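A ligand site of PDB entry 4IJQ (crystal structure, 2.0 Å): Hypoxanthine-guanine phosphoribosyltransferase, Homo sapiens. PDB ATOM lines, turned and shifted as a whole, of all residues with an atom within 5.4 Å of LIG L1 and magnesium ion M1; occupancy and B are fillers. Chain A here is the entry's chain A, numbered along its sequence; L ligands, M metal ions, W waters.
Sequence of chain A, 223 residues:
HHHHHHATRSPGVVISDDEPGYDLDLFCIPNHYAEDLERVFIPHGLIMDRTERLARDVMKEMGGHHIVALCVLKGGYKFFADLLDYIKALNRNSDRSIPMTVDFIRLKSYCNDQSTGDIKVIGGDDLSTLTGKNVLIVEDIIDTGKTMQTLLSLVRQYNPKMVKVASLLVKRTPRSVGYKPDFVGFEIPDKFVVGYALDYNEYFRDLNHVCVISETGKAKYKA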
ATOM      1  N   LEU A 107     -19.677  32.986  21.447  1.00  0.00           N
ATOM      2  CA  LEU A 107     -19.096  33.970  20.542  1.00  0.00           C
ATOM      3  C   LEU A 107     -18.402  33.255  19.392  1.00  0.00           C
ATOM      4  O   LEU A 107     -18.012  32.094  19.514  1.00  0.00           O
ATOM      5  CB  LEU A 107     -18.055  34.817  21.281  1.00  0.00           C
ATOM      6  CG  LEU A 107     -18.469  35.896  22.283  1.00  0.00           C
ATOM      7  CD1 LEU A 107     -19.769  35.550  22.964  1.00  0.00           C
ATOM      8  CD2 LEU A 107     -17.347  36.051  23.296  1.00  0.00           C
ATOM      9  N   LYS A 108     -18.233  33.953  18.270  1.00  0.00           N
ATOM     10  CA  LYS A 108     -17.409  33.463  17.173  1.00  0.00           C
ATOM     11  C   LYS A 108     -16.920  34.622  16.314  1.00  0.00           C
ATOM     12  O   LYS A 108     -15.766  34.652  15.879  1.00  0.00           O
ATOM     13  CB  LYS A 108     -18.174  32.450  16.321  1.00  0.00           C
ATOM     14  CG  LYS A 108     -17.854  30.982  16.614  1.00  0.00           C
ATOM     15  CD  LYS A 108     -16.520  30.577  15.992  1.00  0.00           C
ATOM     16  CE  LYS A 108     -16.186  29.120  16.298  1.00  0.00           C
ATOM     17  NZ  LYS A 108     -16.770  28.160  15.310  1.00  0.00           N
ATOM     18  N   ASP A 140     -11.949  29.502  28.070  1.00  0.00           N
ATOM     19  CA  ASP A 140     -10.931  28.483  27.881  1.00  0.00           C
ATOM     20  C   ASP A 140      -9.555  29.084  27.584  1.00  0.00           C
ATOM     21  O   ASP A 140      -8.569  28.702  28.217  1.00  0.00           O
ATOM     22  CB  ASP A 140     -11.335  27.447  26.789  1.00  0.00           C
ATOM     23  CG  ASP A 140     -11.716  28.114  25.451  1.00  0.00           C
ATOM     24  OD1 ASP A 140     -11.865  29.358  25.396  1.00  0.00           O
ATOM     25  OD2 ASP A 140     -11.870  27.377  24.448  1.00  0.00           O
ATOM     26  N   ILE A 141      -9.480  30.016  26.630  1.00  0.00           N
ATOM     27  CA  ILE A 141      -8.182  30.541  26.223  1.00  0.00           C
ATOM     28  C   ILE A 141      -8.210  31.979  25.698  1.00  0.00           C
ATOM     29  O   ILE A 141      -9.153  32.394  25.022  1.00  0.00           O
ATOM     30  CB  ILE A 141      -7.508  29.595  25.187  1.00  0.00           C
ATOM     31  CG1 ILE A 141      -6.137  30.114  24.774  1.00  0.00           C
ATOM     32  CG2 ILE A 141      -8.395  29.391  23.956  1.00  0.00           C
ATOM     33  CD1 ILE A 141      -5.418  29.112  23.900  1.00  0.00           C
ATOM     34  N   ILE A 142      -7.193  32.743  26.057  1.00  0.00           N
ATOM     35  CA  ILE A 142      -6.995  34.076  25.520  1.00  0.00           C
ATOM     36  C   ILE A 142      -5.699  34.072  24.684  1.00  0.00           C
ATOM     37  O   ILE A 142      -4.642  33.726  25.185  1.00  0.00           O
ATOM     38  CB  ILE A 142      -6.934  35.107  26.652  1.00  0.00           C
ATOM     39  CG1 ILE A 142      -8.298  35.176  27.370  1.00  0.00           C
ATOM     40  CG2 ILE A 142      -6.520  36.479  26.110  1.00  0.00           C
ATOM     41  CD1 ILE A 142      -8.277  36.009  28.614  1.00  0.00           C
ATOM     42  N   ASP A 143      -5.813  34.441  23.413  1.00  0.00           N
ATOM     43  CA  ASP A 143      -4.651  34.532  22.514  1.00  0.00           C
ATOM     44  C   ASP A 143      -4.284  36.001  22.298  1.00  0.00           C
ATOM     45  O   ASP A 143      -3.451  36.526  23.046  1.00  0.00           O
ATOM     46  CB  ASP A 143      -4.930  33.809  21.198  1.00  0.00           C
ATOM     47  CG  ASP A 143      -3.713  33.795  20.241  1.00  0.00           C
ATOM     48  OD1 ASP A 143      -2.597  34.205  20.624  1.00  0.00           O
ATOM     49  OD2 ASP A 143      -3.907  33.366  19.087  1.00  0.00           O
ATOM     50  N   THR A 144      -4.904  36.691  21.333  1.00  0.00           N
ATOM     51  CA  THR A 144      -4.653  38.126  21.173  1.00  0.00           C
ATOM     52  C   THR A 144      -5.313  38.975  22.288  1.00  0.00           C
ATOM     53  O   THR A 144      -4.847  40.102  22.599  1.00  0.00           O
ATOM     54  CB  THR A 144      -5.152  38.677  19.817  1.00  0.00           C
ATOM     55  OG1 THR A 144      -6.587  38.547  19.725  1.00  0.00           O
ATOM     56  CG2 THR A 144      -4.476  37.941  18.644  1.00  0.00           C
ATOM     57  N   GLY A 145      -6.395  38.447  22.870  1.00  0.00           N
ATOM     58  CA  GLY A 145      -7.197  39.201  23.831  1.00  0.00           C
ATOM     59  C   GLY A 145      -8.331  39.993  23.174  1.00  0.00           C
ATOM     60  O   GLY A 145      -9.151  40.643  23.858  1.00  0.00           O
ATOM     61  N   LYS A 146      -8.385  39.945  21.848  1.00  0.00           N
ATOM     62  CA  LYS A 146      -9.336  40.790  21.126  1.00  0.00           C
ATOM     63  C   LYS A 146     -10.764  40.312  21.388  1.00  0.00           C
ATOM     64  O   LYS A 146     -11.659  41.135  21.599  1.00  0.00           O
ATOM     65  CB  LYS A 146      -9.023  40.844  19.621  1.00  0.00           C
ATOM     66  N   THR A 147     -10.973  39.006  21.399  1.00  0.00           N
ATOM     67  CA  THR A 147     -12.296  38.475  21.687  1.00  0.00           C
ATOM     68  C   THR A 147     -12.811  38.864  23.066  1.00  0.00           C
ATOM     69  O   THR A 147     -13.983  39.275  23.217  1.00  0.00           O
ATOM     70  CB  THR A 147     -12.303  36.943  21.586  1.00  0.00           C
ATOM     71  OG1 THR A 147     -11.967  36.570  20.243  1.00  0.00           O
ATOM     72  CG2 THR A 147     -13.661  36.397  21.936  1.00  0.00           C
ATOM     73  N   MET A 148     -11.949  38.723  24.086  1.00  0.00           N
ATOM     74  CA  MET A 148     -12.341  39.057  25.452  1.00  0.00           C
ATOM     75  C   MET A 148     -12.656  40.558  25.587  1.00  0.00           C
ATOM     76  O   MET A 148     -13.648  40.908  26.209  1.00  0.00           O
ATOM     77  CB  MET A 148     -11.299  38.627  26.475  1.00  0.00           C
ATOM     78  CG  MET A 148     -11.786  38.812  27.919  1.00  0.00           C
ATOM     79  SD  MET A 148     -13.372  37.997  28.213  1.00  0.00           S
ATOM     80  CE  MET A 148     -12.980  36.306  27.768  1.00  0.00           C
ATOM     81  N   LYS A 171      -1.993  32.748  26.179  1.00  0.00           N
ATOM     82  CA  LYS A 171      -0.812  32.572  25.327  1.00  0.00           C
ATOM     83  C   LYS A 171       0.178  33.711  25.517  1.00  0.00           C
ATOM     84  O   LYS A 171      -0.219  34.872  25.640  1.00  0.00           O
ATOM     85  CB  LYS A 171      -1.217  32.473  23.860  1.00  0.00           C
ATOM     86  CG  LYS A 171      -1.634  31.072  23.431  1.00  0.00           C
ATOM     87  CD  LYS A 171      -1.834  30.954  21.917  1.00  0.00           C
ATOM     88  CE  LYS A 171      -2.073  29.499  21.555  1.00  0.00           C
ATOM     89  NZ  LYS A 171      -2.561  29.333  20.161  1.00  0.00           N
ATOM     90  N   ILE A 188       1.011  29.736  28.351  1.00  0.00           N
ATOM     91  CA  ILE A 188       1.578  28.772  27.415  1.00  0.00           C
ATOM     92  C   ILE A 188       2.258  29.433  26.206  1.00  0.00           C
ATOM     93  O   ILE A 188       2.018  30.606  25.918  1.00  0.00           O
ATOM     94  CB  ILE A 188       0.500  27.811  26.933  1.00  0.00           C
ATOM     95  CG1 ILE A 188      -0.563  28.561  26.115  1.00  0.00           C
ATOM     96  CG2 ILE A 188      -0.143  27.107  28.136  1.00  0.00           C
ATOM     97  CD1 ILE A 188      -1.490  27.634  25.297  1.00  0.00           C
ATOM     98  N   LYS A 191       1.426  27.926  20.691  1.00  0.00           N
ATOM     99  CA  LYS A 191       1.257  26.675  19.967  1.00  0.00           C
ATOM    100  C   LYS A 191      -0.234  26.396  19.892  1.00  0.00           C
ATOM    101  O   LYS A 191      -0.997  26.813  20.771  1.00  0.00           O
ATOM    102  CB  LYS A 191       1.947  25.526  20.704  1.00  0.00           C
ATOM    103  CG  LYS A 191       3.466  25.500  20.574  1.00  0.00           C
ATOM    104  CD  LYS A 191       4.059  24.343  21.408  1.00  0.00           C
ATOM    105  CE  LYS A 191       5.602  24.317  21.351  1.00  0.00           C
ATOM    106  NZ  LYS A 191       6.216  24.044  22.682  1.00  0.00           N
ATOM    107  N   PHE A 192      -0.660  25.696  18.843  1.00  0.00           N
ATOM    108  CA  PHE A 192      -2.087  25.371  18.753  1.00  0.00           C
ATOM    109  C   PHE A 192      -2.443  24.156  19.626  1.00  0.00           C
ATOM    110  O   PHE A 192      -1.973  23.037  19.364  1.00  0.00           O
ATOM    111  CB  PHE A 192      -2.511  25.119  17.320  1.00  0.00           C
ATOM    112  CG  PHE A 192      -3.979  25.047  17.165  1.00  0.00           C
ATOM    113  CD1 PHE A 192      -4.739  26.206  17.040  1.00  0.00           C
ATOM    114  CD2 PHE A 192      -4.639  23.820  17.204  1.00  0.00           C
ATOM    115  CE1 PHE A 192      -6.124  26.142  16.922  1.00  0.00           C
ATOM    116  CE2 PHE A 192      -6.024  23.756  17.087  1.00  0.00           C
ATOM    117  CZ  PHE A 192      -6.761  24.920  16.956  1.00  0.00           C
ATOM    118  N   VAL A 193      -3.260  24.362  20.657  1.00  0.00           N
ATOM    119  CA  VAL A 193      -3.634  23.278  21.565  1.00  0.00           C
ATOM    120  C   VAL A 193      -5.110  22.888  21.447  1.00  0.00           C
ATOM    121  O   VAL A 193      -5.969  23.706  21.046  1.00  0.00           O
ATOM    122  CB  VAL A 193      -3.310  23.616  23.044  1.00  0.00           C
ATOM    123  CG1 VAL A 193      -1.824  23.655  23.254  1.00  0.00           C
ATOM    124  CG2 VAL A 193      -3.930  24.979  23.418  1.00  0.00           C
ATOM    125  N   VAL A 194      -5.393  21.637  21.796  1.00  0.00           N
ATOM    126  CA  VAL A 194      -6.739  21.079  21.795  1.00  0.00           C
ATOM    127  C   VAL A 194      -6.931  20.257  23.073  1.00  0.00           C
ATOM    128  O   VAL A 194      -5.961  20.009  23.811  1.00  0.00           O
ATOM    129  CB  VAL A 194      -6.997  20.172  20.548  1.00  0.00           C
ATOM    130  CG1 VAL A 194      -6.916  20.987  19.298  1.00  0.00           C
ATOM    131  CG2 VAL A 194      -5.982  19.004  20.510  1.00  0.00           C
ATOM    132  N   LEU A 198     -11.265  22.406  24.290  1.00  0.00           N
ATOM    133  CA  LEU A 198     -10.770  23.163  23.135  1.00  0.00           C
ATOM    134  C   LEU A 198     -10.781  22.296  21.889  1.00  0.00           C
ATOM    135  O   LEU A 198     -10.303  21.142  21.911  1.00  0.00           O
ATOM    136  CB  LEU A 198      -9.349  23.670  23.404  1.00  0.00           C
ATOM    137  CG  LEU A 198      -9.209  24.837  24.373  1.00  0.00           C
ATOM    138  CD1 LEU A 198      -9.410  24.369  25.808  1.00  0.00           C
ATOM    139  CD2 LEU A 198      -7.871  25.519  24.212  1.00  0.00           C
ATOM    140  N   ASP A 199     -11.232  22.836  20.764  1.00  0.00           N
ATOM    141  CA  ASP A 199     -11.368  22.000  19.578  1.00  0.00           C
ATOM    142  C   ASP A 199     -10.489  22.416  18.403  1.00  0.00           C
ATOM    143  O   ASP A 199      -9.946  23.528  18.345  1.00  0.00           O
ATOM    144  CB  ASP A 199     -12.809  22.064  19.074  1.00  0.00           C
ATOM    145  CG  ASP A 199     -13.122  23.391  18.393  1.00  0.00           C
ATOM    146  OD1 ASP A 199     -12.846  24.436  19.032  1.00  0.00           O
ATOM    147  OD2 ASP A 199     -13.615  23.378  17.248  1.00  0.00           O
ATOM    148  N   TYR A 200     -10.430  21.498  17.438  1.00  0.00           N
ATOM    149  CA  TYR A 200      -9.958  21.792  16.114  1.00  0.00           C
ATOM    150  C   TYR A 200     -11.097  21.332  15.203  1.00  0.00           C
ATOM    151  O   TYR A 200     -11.375  20.144  15.118  1.00  0.00           O
ATOM    152  CB  TYR A 200      -8.687  20.999  15.824  1.00  0.00           C
ATOM    153  CG  TYR A 200      -8.216  21.150  14.411  1.00  0.00           C
ATOM    154  CD1 TYR A 200      -7.755  22.372  13.933  1.00  0.00           C
ATOM    155  CD2 TYR A 200      -8.230  20.073  13.534  1.00  0.00           C
ATOM    156  CE1 TYR A 200      -7.321  22.512  12.612  1.00  0.00           C
ATOM    157  CE2 TYR A 200      -7.808  20.197  12.224  1.00  0.00           C
ATOM    158  CZ  TYR A 200      -7.346  21.416  11.770  1.00  0.00           C
ATOM    159  OH  TYR A 200      -6.924  21.513  10.476  1.00  0.00           O
ATOM    160  N   ARG A 205     -12.727  17.879  21.545  1.00  0.00           N
ATOM    161  CA  ARG A 205     -13.364  18.366  22.758  1.00  0.00           C
ATOM    162  C   ARG A 205     -13.487  17.256  23.827  1.00  0.00           C
ATOM    163  O   ARG A 205     -13.411  17.525  25.017  1.00  0.00           O
ATOM    164  CB  ARG A 205     -14.733  18.984  22.458  1.00  0.00           C
ATOM    165  CG  ARG A 205     -14.629  20.253  21.586  1.00  0.00           C
ATOM    166  CD  ARG A 205     -15.844  21.162  21.829  1.00  0.00           C
ATOM    167  NE  ARG A 205     -16.103  22.075  20.725  1.00  0.00           N
ATOM    168  CZ  ARG A 205     -15.599  23.304  20.631  1.00  0.00           C
ATOM    169  NH1 ARG A 205     -14.773  23.787  21.572  1.00  0.00           N
ATOM    170  NH2 ARG A 205     -15.924  24.055  19.573  1.00  0.00           N
HETATM  171  O1  LIG L   1     -13.093  28.156  17.376  1.00  0.00           O
HETATM  172  P1  LIG L   1     -12.540  29.615  17.282  1.00  0.00           P
HETATM  173  O2  LIG L   1     -13.666  30.583  16.803  1.00  0.00           O
HETATM  174  O3  LIG L   1     -11.332  29.691  16.365  1.00  0.00           O
HETATM  175  C1  LIG L   1     -12.052  30.111  18.978  1.00  0.00           C
HETATM  176  O4  LIG L   1     -10.823  29.649  19.419  1.00  0.00           O
HETATM  177  C2  LIG L   1     -10.344  30.337  20.508  1.00  0.00           C
HETATM  178  C3  LIG L   1      -8.983  30.963  20.382  1.00  0.00           C
HETATM  179  C4  LIG L   1      -8.894  32.166  21.266  1.00  0.00           C
HETATM  180  O5  LIG L   1      -8.127  33.235  20.829  1.00  0.00           O
HETATM  181  C5  LIG L   1      -8.909  34.346  20.478  1.00  0.00           C
HETATM  182  P2  LIG L   1      -8.155  35.986  20.710  1.00  0.00           P
HETATM  183  O6  LIG L   1      -6.990  36.095  19.665  1.00  0.00           O
HETATM  184  O7  LIG L   1      -9.310  36.995  20.372  1.00  0.00           O
HETATM  185  O8  LIG L   1      -7.651  36.244  22.110  1.00  0.00           O
HETATM  186  C6  LIG L   1      -8.219  30.981  19.027  1.00  0.00           C
HETATM  187  N1  LIG L   1      -6.983  30.301  19.408  1.00  0.00           N
HETATM  188  C7  LIG L   1      -5.781  30.853  19.662  1.00  0.00           C
HETATM  189  N2  LIG L   1      -4.952  29.860  20.063  1.00  0.00           N
HETATM  190  C8  LIG L   1      -5.683  28.674  20.084  1.00  0.00           C
HETATM  191  C9  LIG L   1      -6.972  28.946  19.691  1.00  0.00           C
HETATM  192  N3  LIG L   1      -7.884  27.926  19.610  1.00  0.00           N
HETATM  193  C10 LIG L   1      -7.525  26.668  19.939  1.00  0.00           C
HETATM  194  N4  LIG L   1      -8.440  25.591  19.874  1.00  0.00           N
HETATM  195  N5  LIG L   1      -6.264  26.398  20.343  1.00  0.00           N
HETATM  196  C11 LIG L   1      -5.331  27.349  20.419  1.00  0.00           C
HETATM  197  O9  LIG L   1      -4.035  27.072  20.823  1.00  0.00           O
HETATM  198  S1  LG2 L   2     -15.328  27.601  20.682  1.00  0.00           S
HETATM  199  O1  LG2 L   2     -14.893  27.508  22.075  1.00  0.00           O
HETATM  200  O2  LG2 L   2     -14.985  28.949  20.187  1.00  0.00           O
HETATM  201  O3  LG2 L   2     -16.788  27.410  20.558  1.00  0.00           O
HETATM  202  O4  LG2 L   2     -14.661  26.568  19.894  1.00  0.00           O
HETATM  203 MG    MG M   1     -12.954  26.404  18.456  1.00  0.00          MG
HETATM  204 MG    MG M   2     -13.186  30.533  24.234  1.00  0.00          MG
HETATM  205  O   HOH W   1      -9.230  37.837  17.833  1.00  0.00           O
HETATM  206  O   HOH W   2      -9.430  28.065  17.158  1.00  0.00           O
HETATM  207  O   HOH W   3     -11.259  25.880  17.248  1.00  0.00           O
HETATM  208  O   HOH W   4     -14.262  25.747  16.853  1.00  0.00           O
HETATM  209  O   HOH W   5     -12.898  29.323  22.528  1.00  0.00           O
HETATM  210  O   HOH W   6     -11.355  26.827  19.831  1.00  0.00           O
HETATM  211  O   HOH W   7     -14.653  32.756  18.394  1.00  0.00           O
HETATM  212  O   HOH W   8      -6.106  34.174  17.819  1.00  0.00           O
HETATM  213  O   HOH W   9     -13.624  32.056  14.873  1.00  0.00           O
HETATM  214  O   HOH W  10      -9.784  36.856  23.848  1.00  0.00           O
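NH2 of Arg 205 lies within salt-bridge range of OD2 of Asp 199 (3.3 Å).
The side-chain amino group (NZ) of Lys 171 sits close to the backbone carbonyl oxygen (O) of Lys 191.
O of Ile 142 lies within hydrogen-bond range of N of Lys 171, at 3.0 Å.
The side-chain hydroxyl (OG1) of Thr 144 sits at hydrogen-bond distance from the backbone NH (N) of Lys 146 (3.1 Å).
The backbone carbonyl oxygen (O) of Asp 199 is in hydrogen-bond range of a nitrogen (N4) of LIG L1, at 3.0 Å.
NZ of Lys 171 lies within hydrogen-bond range of N2 of LIG L1, at 2.5 Å.
An oxygen (O6) of LIG L1 lies within hydrogen-bond range of the backbone NH of Thr 144.
The side-chain hydroxyl of Thr 144 sits at hydrogen-bond distance from an oxygen (O6) of LIG L1.
The backbone NH (N) of Gly 145 is in hydrogen-bond range of an oxygen (O8) of LIG L1 (2.6 Å).
O7 of LIG L1 lies within hydrogen-bond range of N of Thr 147, 2.8 Å away.
OG1 of Thr 147 lies within hydrogen-bond range of O7 of LIG L1 (2.7 Å).
The backbone NH of Val 193 lies within hydrogen-bond range of an oxygen (O9) of LIG L1, 2.8 Å away.
A nitrogen (N4) of LIG L1 lies within hydrogen-bond range of the backbone carbonyl oxygen (O) of Val 193, 3.3 Å away.
An oxygen (O8) of LIG L1 sits at hydrogen-bond distance from the backbone NH (N) of Asp 143 (2.9 Å).
An oxygen (O7) of LIG L1 lies within hydrogen-bond range of the backbone NH (N) of Lys 146.
Residues that only touch magnesium ion M1: Arg 205 (3.9 Å).
Two residues have an atom within 4 Å of magnesium ion M1: Asp 199 and Arg 205.
The nearest printed residue that does not touch magnesium ion M1 is Lys 108 (4.7 Å).
An oxygen (O9) of LIG L1 lies close to the backbone carbonyl oxygen of Lys 191.
CE of Lys 108 touches O2 of LIG L1, 3.0 Å away.
Ile 141 touches LIG L1.
Ile 142 touches LIG L1 (C to O8, 3.9 Å).
Phe 192 touches LIG L1.
13 residues have an atom within 4 Å of LIG L1: Lys 108, Ile 141, Ile 142, Asp 143, Thr 144, Gly 145, Lys 146, Thr 147, Lys 171, Lys 191, Phe 192, Val 193 and Asp 199.
The nearest printed residue that does not touch LIG L1 is Leu 198 (4.1 Å).
Water W1 bridges an oxygen (O7) of LIG L1 and the side-chain hydroxyl (OG1) of Thr 144.
Water W8 bridges OD2 of Asp 143 and O6 of LIG L1.
Water W10 lies within hydrogen-bond range of O8 of LIG L1 (2.8 Å), N of Met 148 (2.9 Å) and N of Thr 147 (3.5 Å).
Water W7 bridges an oxygen (O2) of LIG L1 (2.9 Å) and the backbone carbonyl oxygen of Lys 108 (3.3 Å).
Magnesium ion M1 is bound by the side-chain carboxylate of Asp 199, an oxygen (O1) of LIG L1, water W3, water W6, water W4 and an oxygen (O4) of LG2 L2.
Magnesium ion M1 has six donor atoms within binding distance.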
